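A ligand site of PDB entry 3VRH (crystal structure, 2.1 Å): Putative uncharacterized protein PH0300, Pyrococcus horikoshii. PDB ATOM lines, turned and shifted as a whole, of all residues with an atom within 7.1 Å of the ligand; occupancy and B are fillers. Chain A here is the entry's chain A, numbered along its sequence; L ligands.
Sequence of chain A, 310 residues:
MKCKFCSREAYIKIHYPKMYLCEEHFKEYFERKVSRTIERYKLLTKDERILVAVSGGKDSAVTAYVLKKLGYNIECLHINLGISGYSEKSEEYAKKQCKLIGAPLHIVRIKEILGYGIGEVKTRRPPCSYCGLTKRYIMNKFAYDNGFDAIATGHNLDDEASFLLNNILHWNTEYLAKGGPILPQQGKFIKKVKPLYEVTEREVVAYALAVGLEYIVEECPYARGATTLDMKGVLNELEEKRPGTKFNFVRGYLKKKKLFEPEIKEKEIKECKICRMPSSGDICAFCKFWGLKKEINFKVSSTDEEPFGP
Gly 57 touches the ligand.
Asp 59 touches the ligand.
Thr 153 touches the ligand (CA to O4, 3.4 Å).
Gly 154 touches the ligand (N to C5, 3.0 Å).
His 155 touches the ligand (NE2 to O1, 3.8 Å).
Asp 159 touches the ligand (OD2 to O2, 3.6 Å).
Hydrophobic or aromatic side chains within 4 Å of the ligand: Ala 53 and His 155.
Of the 27 residues printed, 9 come within 4 Å of the ligand.
The nearest printed residue that does not touch the ligand is Ala 152 (4.02 Å).
The side-chain hydroxyl (OG1) of Thr 63 sits at hydrogen-bond distance from the backbone carbonyl oxygen (O) of Asp 59, 2.7 Å away.
The side-chain amino group (NZ) of Lys 58 is in salt-bridge range of the side-chain carboxylate (OD2) of Asp 59, at 3.1 Å.
The side-chain carboxylate (OD1) of Asp 159 lies within salt-bridge range of the side-chain amino group (NZ) of Lys 232 (2.6 Å).
The side-chain hydroxyl (OG) of Ser 60 sits at hydrogen-bond distance from the backbone NH (N) of Ser 55 (3.2 Å).
OG1 of Thr 153 lies within hydrogen-bond range of ND1 of His 155, at 2.9 Å.
The backbone NH (N) of Gly 57 is in hydrogen-bond range of the side-chain hydroxyl (OG) of Ser 55.
The side-chain amide nitrogen (ND2) of Asn 156 lies within hydrogen-bond range of the side-chain carboxylate (OD1) of Asp 59.
The side-chain carboxylate (OD2) of Asp 159 sits at hydrogen-bond distance from the backbone NH (N) of Asn 156 (2.9 Å).
An oxygen (O4) of the ligand is in hydrogen-bond range of the backbone carbonyl oxygen (O) of Ala 53, 2.8 Å away.
The backbone NH (N) of Ser 60 sits at hydrogen-bond distance from an oxygen (O3) of the ligand (3.0 Å).
O3 of the ligand lies within hydrogen-bond range of OG of Ser 60.
An oxygen (O3) of the ligand is in hydrogen-bond range of the side-chain hydroxyl (OG) of Ser 55 (2.9 Å).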
ATOM      1  N   LEU A  51       6.651  23.078  20.601  1.00  0.00           N
ATOM      2  CA  LEU A  51       5.735  22.499  21.573  1.00  0.00           C
ATOM      3  C   LEU A  51       4.507  23.399  21.718  1.00  0.00           C
ATOM      4  O   LEU A  51       4.647  24.599  21.912  1.00  0.00           O
ATOM      5  CB  LEU A  51       6.434  22.352  22.914  1.00  0.00           C
ATOM      6  CG  LEU A  51       5.547  21.767  24.014  1.00  0.00           C
ATOM      7  CD1 LEU A  51       5.278  20.296  23.726  1.00  0.00           C
ATOM      8  CD2 LEU A  51       6.119  21.978  25.413  1.00  0.00           C
ATOM      9  N   VAL A  52       3.309  22.817  21.612  1.00  0.00           N
ATOM     10  CA  VAL A  52       2.074  23.590  21.856  1.00  0.00           C
ATOM     11  C   VAL A  52       1.381  23.046  23.097  1.00  0.00           C
ATOM     12  O   VAL A  52       1.093  21.840  23.202  1.00  0.00           O
ATOM     13  CB  VAL A  52       1.095  23.558  20.654  1.00  0.00           C
ATOM     14  CG1 VAL A  52      -0.153  24.376  20.965  1.00  0.00           C
ATOM     15  CG2 VAL A  52       1.775  24.068  19.405  1.00  0.00           C
ATOM     16  N   ALA A  53       1.138  23.928  24.064  1.00  0.00           N
ATOM     17  CA  ALA A  53       0.503  23.539  25.319  1.00  0.00           C
ATOM     18  C   ALA A  53      -0.973  23.517  25.074  1.00  0.00           C
ATOM     19  O   ALA A  53      -1.587  24.556  24.884  1.00  0.00           O
ATOM     20  CB  ALA A  53       0.824  24.557  26.425  1.00  0.00           C
ATOM     21  N   VAL A  54      -1.556  22.333  25.068  1.00  0.00           N
ATOM     22  CA  VAL A  54      -2.968  22.220  24.709  1.00  0.00           C
ATOM     23  C   VAL A  54      -3.858  21.971  25.937  1.00  0.00           C
ATOM     24  O   VAL A  54      -3.776  20.918  26.576  1.00  0.00           O
ATOM     25  CB  VAL A  54      -3.182  21.192  23.563  1.00  0.00           C
ATOM     26  CG1 VAL A  54      -2.329  21.563  22.369  1.00  0.00           C
ATOM     27  CG2 VAL A  54      -2.790  19.811  24.004  1.00  0.00           C
ATOM     28  N   SER A  55      -4.675  22.960  26.284  1.00  0.00           N
ATOM     29  CA  SER A  55      -5.529  22.889  27.466  1.00  0.00           C
ATOM     30  C   SER A  55      -6.820  22.116  27.185  1.00  0.00           C
ATOM     31  O   SER A  55      -7.545  21.768  28.106  1.00  0.00           O
ATOM     32  CB  SER A  55      -5.930  24.300  27.886  1.00  0.00           C
ATOM     33  OG  SER A  55      -6.655  24.908  26.807  1.00  0.00           O
ATOM     34  N   GLY A  56      -7.109  21.874  25.908  1.00  0.00           N
ATOM     35  CA  GLY A  56      -8.429  21.426  25.519  1.00  0.00           C
ATOM     36  C   GLY A  56      -9.333  22.588  25.101  1.00  0.00           C
ATOM     37  O   GLY A  56     -10.404  22.366  24.555  1.00  0.00           O
ATOM     38  N   GLY A  57      -8.892  23.820  25.367  1.00  0.00           N
ATOM     39  CA  GLY A  57      -9.595  25.032  24.925  1.00  0.00           C
ATOM     40  C   GLY A  57      -9.440  25.260  23.438  1.00  0.00           C
ATOM     41  O   GLY A  57      -8.603  24.624  22.777  1.00  0.00           O
ATOM     42  N   LYS A  58     -10.261  26.131  22.863  1.00  0.00           N
ATOM     43  CA  LYS A  58     -10.242  26.341  21.413  1.00  0.00           C
ATOM     44  C   LYS A  58      -8.930  26.946  20.895  1.00  0.00           C
ATOM     45  O   LYS A  58      -8.528  26.686  19.768  1.00  0.00           O
ATOM     46  CB  LYS A  58     -11.401  27.254  20.978  1.00  0.00           C
ATOM     47  CG  LYS A  58     -11.230  28.715  21.482  1.00  0.00           C
ATOM     48  CD  LYS A  58     -12.399  29.615  21.144  1.00  0.00           C
ATOM     49  CE  LYS A  58     -12.118  31.058  21.574  1.00  0.00           C
ATOM     50  NZ  LYS A  58     -11.855  31.202  23.048  1.00  0.00           N
ATOM     51  N   ASP A  59      -8.289  27.779  21.718  1.00  0.00           N
ATOM     52  CA  ASP A  59      -7.195  28.626  21.241  1.00  0.00           C
ATOM     53  C   ASP A  59      -5.903  27.850  21.009  1.00  0.00           C
ATOM     54  O   ASP A  59      -5.275  27.958  19.969  1.00  0.00           O
ATOM     55  CB  ASP A  59      -6.979  29.793  22.209  1.00  0.00           C
ATOM     56  CG  ASP A  59      -8.276  30.593  22.435  1.00  0.00           C
ATOM     57  OD1 ASP A  59      -8.697  31.302  21.499  1.00  0.00           O
ATOM     58  OD2 ASP A  59      -8.895  30.472  23.508  1.00  0.00           O
ATOM     59  N   SER A  60      -5.510  27.062  22.004  1.00  0.00           N
ATOM     60  CA  SER A  60      -4.368  26.189  21.852  1.00  0.00           C
ATOM     61  C   SER A  60      -4.670  25.094  20.827  1.00  0.00           C
ATOM     62  O   SER A  60      -3.766  24.661  20.106  1.00  0.00           O
ATOM     63  CB  SER A  60      -3.970  25.600  23.200  1.00  0.00           C
ATOM     64  OG  SER A  60      -5.069  25.015  23.866  1.00  0.00           O
ATOM     65  N   ALA A  61      -5.918  24.665  20.730  1.00  0.00           N
ATOM     66  CA  ALA A  61      -6.283  23.649  19.744  1.00  0.00           C
ATOM     67  C   ALA A  61      -6.095  24.139  18.319  1.00  0.00           C
ATOM     68  O   ALA A  61      -5.565  23.428  17.481  1.00  0.00           O
ATOM     69  CB  ALA A  61      -7.731  23.187  19.951  1.00  0.00           C
ATOM     70  N   VAL A  62      -6.583  25.350  18.047  1.00  0.00           N
ATOM     71  CA  VAL A  62      -6.492  25.921  16.710  1.00  0.00           C
ATOM     72  C   VAL A  62      -5.026  26.228  16.408  1.00  0.00           C
ATOM     73  O   VAL A  62      -4.564  26.098  15.276  1.00  0.00           O
ATOM     74  CB  VAL A  62      -7.397  27.197  16.607  1.00  0.00           C
ATOM     75  CG1 VAL A  62      -7.013  28.075  15.404  1.00  0.00           C
ATOM     76  CG2 VAL A  62      -8.873  26.807  16.522  1.00  0.00           C
ATOM     77  N   THR A  63      -4.285  26.624  17.450  1.00  0.00           N
ATOM     78  CA  THR A  63      -2.878  26.932  17.283  1.00  0.00           C
ATOM     79  C   THR A  63      -2.165  25.681  16.760  1.00  0.00           C
ATOM     80  O   THR A  63      -1.523  25.724  15.721  1.00  0.00           O
ATOM     81  CB  THR A  63      -2.209  27.383  18.585  1.00  0.00           C
ATOM     82  OG1 THR A  63      -2.795  28.611  19.030  1.00  0.00           O
ATOM     83  CG2 THR A  63      -0.717  27.613  18.388  1.00  0.00           C
ATOM     84  N   LEU A  77       1.540  19.326  24.441  1.00  0.00           N
ATOM     85  CA  LEU A  77       1.584  18.974  25.841  1.00  0.00           C
ATOM     86  C   LEU A  77       0.286  19.402  26.505  1.00  0.00           C
ATOM     87  O   LEU A  77      -0.108  20.569  26.403  1.00  0.00           O
ATOM     88  CB  LEU A  77       2.759  19.664  26.531  1.00  0.00           C
ATOM     89  CG  LEU A  77       2.715  19.669  28.064  1.00  0.00           C
ATOM     90  CD1 LEU A  77       2.894  18.271  28.622  1.00  0.00           C
ATOM     91  CD2 LEU A  77       3.773  20.622  28.637  1.00  0.00           C
ATOM     92  N   GLN A  97      -8.571  16.313  20.138  1.00  0.00           N
ATOM     93  CA  GLN A  97      -7.974  17.339  19.295  1.00  0.00           C
ATOM     94  C   GLN A  97      -6.651  16.892  18.660  1.00  0.00           C
ATOM     95  O   GLN A  97      -6.444  17.069  17.459  1.00  0.00           O
ATOM     96  CB  GLN A  97      -7.754  18.630  20.094  1.00  0.00           C
ATOM     97  CG  GLN A  97      -9.045  19.366  20.462  1.00  0.00           C
ATOM     98  CD  GLN A  97      -8.853  20.339  21.592  1.00  0.00           C
ATOM     99  OE1 GLN A  97      -7.736  20.568  22.077  1.00  0.00           O
ATOM    100  NE2 GLN A  97      -9.959  20.935  22.045  1.00  0.00           N
ATOM    101  N   LYS A 135       1.510  26.011  35.777  1.00  0.00           N
ATOM    102  CA  LYS A 135       1.409  25.615  34.376  1.00  0.00           C
ATOM    103  C   LYS A 135       2.557  26.194  33.527  1.00  0.00           C
ATOM    104  O   LYS A 135       3.128  25.499  32.678  1.00  0.00           O
ATOM    105  CB  LYS A 135       0.034  26.007  33.801  1.00  0.00           C
ATOM    106  CG  LYS A 135      -0.151  25.541  32.357  1.00  0.00           C
ATOM    107  CD  LYS A 135      -1.469  26.087  31.725  1.00  0.00           C
ATOM    108  CE  LYS A 135      -1.631  25.583  30.278  1.00  0.00           C
ATOM    109  NZ  LYS A 135      -2.868  26.072  29.593  1.00  0.00           N
ATOM    110  N   MET A 139       5.340  23.958  31.499  1.00  0.00           N
ATOM    111  CA  MET A 139       5.449  24.118  30.060  1.00  0.00           C
ATOM    112  C   MET A 139       6.903  24.374  29.690  1.00  0.00           C
ATOM    113  O   MET A 139       7.436  23.770  28.768  1.00  0.00           O
ATOM    114  CB  MET A 139       4.620  25.300  29.540  1.00  0.00           C
ATOM    115  CG  MET A 139       3.118  25.087  29.474  1.00  0.00           C
ATOM    116  SD  MET A 139       2.333  26.700  29.270  1.00  0.00           S
ATOM    117  CE  MET A 139       3.136  27.245  27.768  1.00  0.00           C
ATOM    118  N   ILE A 151       7.977  27.311  22.317  1.00  0.00           N
ATOM    119  CA  ILE A 151       6.641  27.018  22.805  1.00  0.00           C
ATOM    120  C   ILE A 151       5.702  27.988  22.124  1.00  0.00           C
ATOM    121  O   ILE A 151       5.919  29.208  22.169  1.00  0.00           O
ATOM    122  CB  ILE A 151       6.567  27.227  24.323  1.00  0.00           C
ATOM    123  CG1 ILE A 151       7.443  26.207  25.030  1.00  0.00           C
ATOM    124  CG2 ILE A 151       5.132  27.178  24.817  1.00  0.00           C
ATOM    125  CD1 ILE A 151       7.637  26.498  26.489  1.00  0.00           C
ATOM    126  N   ALA A 152       4.667  27.475  21.469  1.00  0.00           N
ATOM    127  CA  ALA A 152       3.634  28.323  20.876  1.00  0.00           C
ATOM    128  C   ALA A 152       2.363  28.251  21.733  1.00  0.00           C
ATOM    129  O   ALA A 152       1.926  27.162  22.090  1.00  0.00           O
ATOM    130  CB  ALA A 152       3.344  27.896  19.461  1.00  0.00           C
ATOM    131  N   THR A 153       1.804  29.418  22.080  1.00  0.00           N
ATOM    132  CA  THR A 153       0.539  29.489  22.800  1.00  0.00           C
ATOM    133  C   THR A 153      -0.571  30.080  21.916  1.00  0.00           C
ATOM    134  O   THR A 153      -0.307  30.562  20.818  1.00  0.00           O
ATOM    135  CB  THR A 153       0.679  30.288  24.109  1.00  0.00           C
ATOM    136  OG1 THR A 153       1.003  31.640  23.805  1.00  0.00           O
ATOM    137  CG2 THR A 153       1.798  29.693  24.983  1.00  0.00           C
ATOM    138  N   GLY A 154      -1.807  30.023  22.390  1.00  0.00           N
ATOM    139  CA  GLY A 154      -2.969  30.341  21.579  1.00  0.00           C
ATOM    140  C   GLY A 154      -3.577  31.735  21.774  1.00  0.00           C
ATOM    141  O   GLY A 154      -4.639  32.021  21.232  1.00  0.00           O
ATOM    142  N   HIS A 155      -2.897  32.575  22.530  1.00  0.00           N
ATOM    143  CA  HIS A 155      -3.324  33.964  22.738  1.00  0.00           C
ATOM    144  C   HIS A 155      -3.598  34.668  21.429  1.00  0.00           C
ATOM    145  O   HIS A 155      -2.740  34.738  20.549  1.00  0.00           O
ATOM    146  CB  HIS A 155      -2.237  34.738  23.494  1.00  0.00           C
ATOM    147  CG  HIS A 155      -1.914  34.198  24.843  1.00  0.00           C
ATOM    148  ND1 HIS A 155      -1.237  33.008  25.025  1.00  0.00           N
ATOM    149  CD2 HIS A 155      -2.164  34.679  26.087  1.00  0.00           C
ATOM    150  CE1 HIS A 155      -1.082  32.778  26.320  1.00  0.00           C
ATOM    151  NE2 HIS A 155      -1.645  33.775  26.986  1.00  0.00           N
ATOM    152  N   ASN A 156      -4.809  35.183  21.291  1.00  0.00           N
ATOM    153  CA  ASN A 156      -5.194  35.870  20.079  1.00  0.00           C
ATOM    154  C   ASN A 156      -5.301  37.372  20.342  1.00  0.00           C
ATOM    155  O   ASN A 156      -4.970  37.835  21.430  1.00  0.00           O
ATOM    156  CB  ASN A 156      -6.509  35.278  19.540  1.00  0.00           C
ATOM    157  CG  ASN A 156      -7.679  35.437  20.513  1.00  0.00           C
ATOM    158  OD1 ASN A 156      -7.922  36.546  21.014  1.00  0.00           O
ATOM    159  ND2 ASN A 156      -8.381  34.350  20.796  1.00  0.00           N
ATOM    160  N   ASP A 159      -7.220  38.382  23.444  1.00  0.00           N
ATOM    161  CA  ASP A 159      -6.455  38.105  24.662  1.00  0.00           C
ATOM    162  C   ASP A 159      -5.429  39.177  24.956  1.00  0.00           C
ATOM    163  O   ASP A 159      -5.364  39.681  26.081  1.00  0.00           O
ATOM    164  CB  ASP A 159      -5.778  36.734  24.575  1.00  0.00           C
ATOM    165  CG  ASP A 159      -6.780  35.622  24.378  1.00  0.00           C
ATOM    166  OD1 ASP A 159      -7.806  35.667  25.092  1.00  0.00           O
ATOM    167  OD2 ASP A 159      -6.580  34.744  23.501  1.00  0.00           O
ATOM    168  N   ILE A 216     -13.375  22.600  25.262  1.00  0.00           N
ATOM    169  CA  ILE A 216     -13.992  23.073  26.494  1.00  0.00           C
ATOM    170  C   ILE A 216     -13.937  24.594  26.533  1.00  0.00           C
ATOM    171  O   ILE A 216     -13.120  25.217  25.850  1.00  0.00           O
ATOM    172  CB  ILE A 216     -13.242  22.508  27.715  1.00  0.00           C
ATOM    173  CG1 ILE A 216     -11.902  23.219  27.888  1.00  0.00           C
ATOM    174  CG2 ILE A 216     -13.005  21.010  27.565  1.00  0.00           C
ATOM    175  CD1 ILE A 216     -10.921  22.485  28.791  1.00  0.00           C
ATOM    176  N   GLU A 219     -10.655  26.244  31.297  1.00  0.00           N
ATOM    177  CA  GLU A 219      -9.565  25.372  31.753  1.00  0.00           C
ATOM    178  C   GLU A 219      -9.553  25.259  33.277  1.00  0.00           C
ATOM    179  O   GLU A 219      -9.593  24.158  33.830  1.00  0.00           O
ATOM    180  CB  GLU A 219      -8.220  25.922  31.248  1.00  0.00           C
ATOM    181  CG  GLU A 219      -7.016  25.125  31.701  1.00  0.00           C
ATOM    182  CD  GLU A 219      -5.691  25.676  31.159  1.00  0.00           C
ATOM    183  OE1 GLU A 219      -5.701  26.787  30.558  1.00  0.00           O
ATOM    184  OE2 GLU A 219      -4.659  24.983  31.317  1.00  0.00           O
ATOM    185  N   LYS A 232     -12.813  41.836  28.029  1.00  0.00           N
ATOM    186  CA  LYS A 232     -13.178  41.502  26.667  1.00  0.00           C
ATOM    187  C   LYS A 232     -14.530  42.123  26.319  1.00  0.00           C
ATOM    188  O   LYS A 232     -14.718  42.584  25.191  1.00  0.00           O
ATOM    189  CB  LYS A 232     -13.178  39.986  26.426  1.00  0.00           C
ATOM    190  CG  LYS A 232     -11.773  39.381  26.329  1.00  0.00           C
ATOM    191  CD  LYS A 232     -11.799  37.869  26.262  1.00  0.00           C
ATOM    192  CE  LYS A 232     -10.392  37.309  25.968  1.00  0.00           C
ATOM    193  NZ  LYS A 232     -10.391  35.899  25.425  1.00  0.00           N
HETATM  194  N1  LIG L   1      -3.769  29.029  25.724  1.00  0.00           N
HETATM  195  C1  LIG L   1      -4.403  30.250  25.081  1.00  0.00           C
HETATM  196  C2  LIG L   1      -4.960  31.241  26.032  1.00  0.00           C
HETATM  197  O1  LIG L   1      -4.453  31.294  27.176  1.00  0.00           O
HETATM  198  O2  LIG L   1      -5.931  31.967  25.715  1.00  0.00           O
HETATM  199  C3  LIG L   1      -4.772  27.947  25.928  1.00  0.00           C
HETATM  200  C4  LIG L   1      -6.083  27.990  25.116  1.00  0.00           C
HETATM  201  O3  LIG L   1      -6.648  26.982  24.762  1.00  0.00           O
HETATM  202  C5  LIG L   1      -2.690  28.533  24.867  1.00  0.00           C
HETATM  203  C6  LIG L   1      -1.830  27.534  25.522  1.00  0.00           C
HETATM  204  O4  LIG L   1      -0.767  27.252  25.073  1.00  0.00           O
